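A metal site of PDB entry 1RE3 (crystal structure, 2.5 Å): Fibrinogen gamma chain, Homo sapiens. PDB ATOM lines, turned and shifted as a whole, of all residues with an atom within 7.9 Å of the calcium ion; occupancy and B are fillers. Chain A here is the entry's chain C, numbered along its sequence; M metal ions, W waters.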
ATOM      1  N   SER A 218      31.682 -11.470   2.348  1.00  0.00           N
ATOM      2  CA  SER A 218      32.011 -10.211   2.996  1.00  0.00           C
ATOM      3  C   SER A 218      33.427 -10.216   3.564  1.00  0.00           C
ATOM      4  O   SER A 218      33.925 -11.243   4.002  1.00  0.00           O
ATOM      5  CB  SER A 218      31.037  -9.898   4.134  1.00  0.00           C
ATOM      6  OG  SER A 218      29.784  -9.448   3.658  1.00  0.00           O
ATOM      7  N   ASN A 222      34.587  -4.863   2.370  1.00  0.00           N
ATOM      8  CA  ASN A 222      33.559  -5.090   1.363  1.00  0.00           C
ATOM      9  C   ASN A 222      32.395  -5.801   2.042  1.00  0.00           C
ATOM     10  O   ASN A 222      32.223  -7.018   1.931  1.00  0.00           O
ATOM     11  CB  ASN A 222      34.121  -5.952   0.221  1.00  0.00           C
ATOM     12  CG  ASN A 222      33.425  -5.700  -1.120  1.00  0.00           C
ATOM     13  OD1 ASN A 222      34.089  -5.454  -2.132  1.00  0.00           O
ATOM     14  ND2 ASN A 222      32.098  -5.767  -1.141  1.00  0.00           N
ATOM     15  N   ASP A 223      31.594  -5.001   2.756  1.00  0.00           N
ATOM     16  CA  ASP A 223      30.435  -5.459   3.518  1.00  0.00           C
ATOM     17  C   ASP A 223      29.236  -5.765   2.635  1.00  0.00           C
ATOM     18  O   ASP A 223      28.658  -4.856   2.030  1.00  0.00           O
ATOM     19  CB  ASP A 223      30.048  -4.385   4.547  1.00  0.00           C
ATOM     20  CG  ASP A 223      28.951  -4.833   5.499  1.00  0.00           C
ATOM     21  OD1 ASP A 223      28.043  -5.582   5.070  1.00  0.00           O
ATOM     22  OD2 ASP A 223      29.001  -4.414   6.669  1.00  0.00           O
ATOM     23  N   ASN A 224      28.843  -7.035   2.565  1.00  0.00           N
ATOM     24  CA  ASN A 224      27.692  -7.403   1.762  1.00  0.00           C
ATOM     25  C   ASN A 224      26.758  -8.304   2.570  1.00  0.00           C
ATOM     26  O   ASN A 224      26.102  -9.176   2.014  1.00  0.00           O
ATOM     27  CB  ASN A 224      28.145  -8.120   0.483  1.00  0.00           C
ATOM     28  CG  ASN A 224      29.159  -7.317  -0.328  1.00  0.00           C
ATOM     29  OD1 ASN A 224      30.312  -7.702  -0.453  1.00  0.00           O
ATOM     30  ND2 ASN A 224      28.724  -6.179  -0.866  1.00  0.00           N
ATOM     31  N   ASP A 225      26.692  -8.084   3.873  1.00  0.00           N
ATOM     32  CA  ASP A 225      25.857  -8.900   4.732  1.00  0.00           C
ATOM     33  C   ASP A 225      24.468  -8.315   4.992  1.00  0.00           C
ATOM     34  O   ASP A 225      24.085  -7.294   4.427  1.00  0.00           O
ATOM     35  CB  ASP A 225      26.565  -9.163   6.068  1.00  0.00           C
ATOM     36  CG  ASP A 225      26.839  -7.890   6.853  1.00  0.00           C
ATOM     37  OD1 ASP A 225      25.889  -7.085   7.007  1.00  0.00           O
ATOM     38  OD2 ASP A 225      27.976  -7.711   7.326  1.00  0.00           O
ATOM     39  N   LYS A 226      23.717  -8.986   5.870  1.00  0.00           N
ATOM     40  CA  LYS A 226      22.351  -8.582   6.235  1.00  0.00           C
ATOM     41  C   LYS A 226      22.299  -7.898   7.603  1.00  0.00           C
ATOM     42  O   LYS A 226      21.270  -7.906   8.286  1.00  0.00           O
ATOM     43  CB  LYS A 226      21.444  -9.814   6.248  1.00  0.00           C
ATOM     44  CG  LYS A 226      21.419 -10.599   4.941  1.00  0.00           C
ATOM     45  CD  LYS A 226      20.833  -9.757   3.818  1.00  0.00           C
ATOM     46  CE  LYS A 226      20.726 -10.541   2.528  1.00  0.00           C
ATOM     47  NZ  LYS A 226      19.884  -9.809   1.530  1.00  0.00           N
ATOM     48  N   PHE A 227      23.417  -7.294   7.991  1.00  0.00           N
ATOM     49  CA  PHE A 227      23.547  -6.625   9.273  1.00  0.00           C
ATOM     50  C   PHE A 227      23.805  -5.139   9.023  1.00  0.00           C
ATOM     51  O   PHE A 227      24.436  -4.771   8.038  1.00  0.00           O
ATOM     52  CB  PHE A 227      24.706  -7.278  10.041  1.00  0.00           C
ATOM     53  CG  PHE A 227      25.039  -6.644  11.361  1.00  0.00           C
ATOM     54  CD1 PHE A 227      24.055  -6.118  12.185  1.00  0.00           C
ATOM     55  CD2 PHE A 227      26.364  -6.637  11.817  1.00  0.00           C
ATOM     56  CE1 PHE A 227      24.372  -5.584  13.432  1.00  0.00           C
ATOM     57  CE2 PHE A 227      26.703  -6.109  13.067  1.00  0.00           C
ATOM     58  CZ  PHE A 227      25.697  -5.582  13.880  1.00  0.00           C
ATOM     59  N   GLU A 228      23.287  -4.276   9.885  1.00  0.00           N
ATOM     60  CA  GLU A 228      23.488  -2.836   9.725  1.00  0.00           C
ATOM     61  C   GLU A 228      24.934  -2.551  10.066  1.00  0.00           C
ATOM     62  O   GLU A 228      25.467  -1.493   9.734  1.00  0.00           O
ATOM     63  CB  GLU A 228      22.554  -2.020  10.639  1.00  0.00           C
ATOM     64  CG  GLU A 228      21.832  -2.829  11.702  1.00  0.00           C
ATOM     65  CD  GLU A 228      20.932  -3.920  11.124  1.00  0.00           C
ATOM     66  OE1 GLU A 228      20.048  -3.596  10.290  1.00  0.00           O
ATOM     67  OE2 GLU A 228      21.103  -5.114  11.499  1.00  0.00           O
ATOM     68  N   GLY A 229      25.568  -3.520  10.727  1.00  0.00           N
ATOM     69  CA  GLY A 229      26.965  -3.394  11.092  1.00  0.00           C
ATOM     70  C   GLY A 229      27.830  -4.184  10.128  1.00  0.00           C
ATOM     71  O   GLY A 229      27.356  -4.642   9.072  1.00  0.00           O
ATOM     72  N   ASN A 230      29.096  -4.372  10.480  1.00  0.00           N
ATOM     73  CA  ASN A 230      30.036  -5.095   9.631  1.00  0.00           C
ATOM     74  C   ASN A 230      30.482  -6.404  10.280  1.00  0.00           C
ATOM     75  O   ASN A 230      31.466  -6.444  11.017  1.00  0.00           O
ATOM     76  CB  ASN A 230      31.249  -4.192   9.362  1.00  0.00           C
ATOM     77  CG  ASN A 230      32.087  -4.661   8.186  1.00  0.00           C
ATOM     78  OD1 ASN A 230      32.719  -3.843   7.509  1.00  0.00           O
ATOM     79  ND2 ASN A 230      32.111  -5.973   7.941  1.00  0.00           N
ATOM     80  N   CYS A 231      29.752  -7.484   9.997  1.00  0.00           N
ATOM     81  CA  CYS A 231      30.100  -8.791  10.561  1.00  0.00           C
ATOM     82  C   CYS A 231      31.562  -9.114  10.350  1.00  0.00           C
ATOM     83  O   CYS A 231      32.310  -9.337  11.307  1.00  0.00           O
ATOM     84  CB  CYS A 231      29.273  -9.908   9.921  1.00  0.00           C
ATOM     85  SG  CYS A 231      27.493  -9.884  10.297  1.00  0.00           S
ATOM     86  N   ALA A 232      31.962  -9.157   9.082  1.00  0.00           N
ATOM     87  CA  ALA A 232      33.322  -9.489   8.680  1.00  0.00           C
ATOM     88  C   ALA A 232      34.386  -8.742   9.476  1.00  0.00           C
ATOM     89  O   ALA A 232      35.370  -9.333   9.912  1.00  0.00           O
ATOM     90  CB  ALA A 232      33.514  -9.225   7.189  1.00  0.00           C
ATOM     91  N   MET A 241      28.683 -13.840   5.316  1.00  0.00           N
ATOM     92  CA  MET A 241      27.991 -13.337   6.492  1.00  0.00           C
ATOM     93  C   MET A 241      26.519 -12.988   6.295  1.00  0.00           C
ATOM     94  O   MET A 241      26.127 -12.417   5.275  1.00  0.00           O
ATOM     95  CB  MET A 241      28.729 -12.111   7.027  1.00  0.00           C
ATOM     96  CG  MET A 241      30.144 -12.400   7.494  1.00  0.00           C
ATOM     97  SD  MET A 241      30.214 -13.465   8.970  1.00  0.00           S
ATOM     98  CE  MET A 241      31.967 -13.349   9.422  1.00  0.00           C
ATOM     99  N   ASN A 242      25.720 -13.325   7.303  1.00  0.00           N
ATOM    100  CA  ASN A 242      24.289 -13.016   7.320  1.00  0.00           C
ATOM    101  C   ASN A 242      24.183 -11.944   8.418  1.00  0.00           C
ATOM    102  O   ASN A 242      24.431 -10.761   8.167  1.00  0.00           O
ATOM    103  CB  ASN A 242      23.477 -14.247   7.708  1.00  0.00           C
ATOM    104  CG  ASN A 242      22.000 -14.115   7.387  1.00  0.00           C
ATOM    105  OD1 ASN A 242      21.445 -13.017   7.417  1.00  0.00           O
ATOM    106  ND2 ASN A 242      21.339 -15.236   7.105  1.00  0.00           N
HETATM  107 CA    CA M   1      26.572  -4.709   6.923  1.00  0.00          CA
HETATM  108  O   HOH W   1      25.012  -5.050   5.211  1.00  0.00           O
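The backbone NH (N) of Cys 231 sits at hydrogen-bond distance from the side-chain carboxylate (OD2) of Asp 225, 3.2 Å away. OG of Ser 218 sits at hydrogen-bond distance from N of Asp 225, 3.4 Å away.
The calcium ion is bound by the backbone carbonyl oxygen (O) of Gly 229 (2.3 Å), water W1 (2.3 Å), the backbone carbonyl oxygen (O) of Phe 227 (2.4 Å), the side-chain carboxylate (OD2) of Asp 223 (2.5 Å), the side-chain carboxylate (OD1) of Asp 225 (2.5 Å) and the side-chain carboxylate (OD1) of Asp 223 (2.5 Å). The calcium ion has six donor atoms within binding distance.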
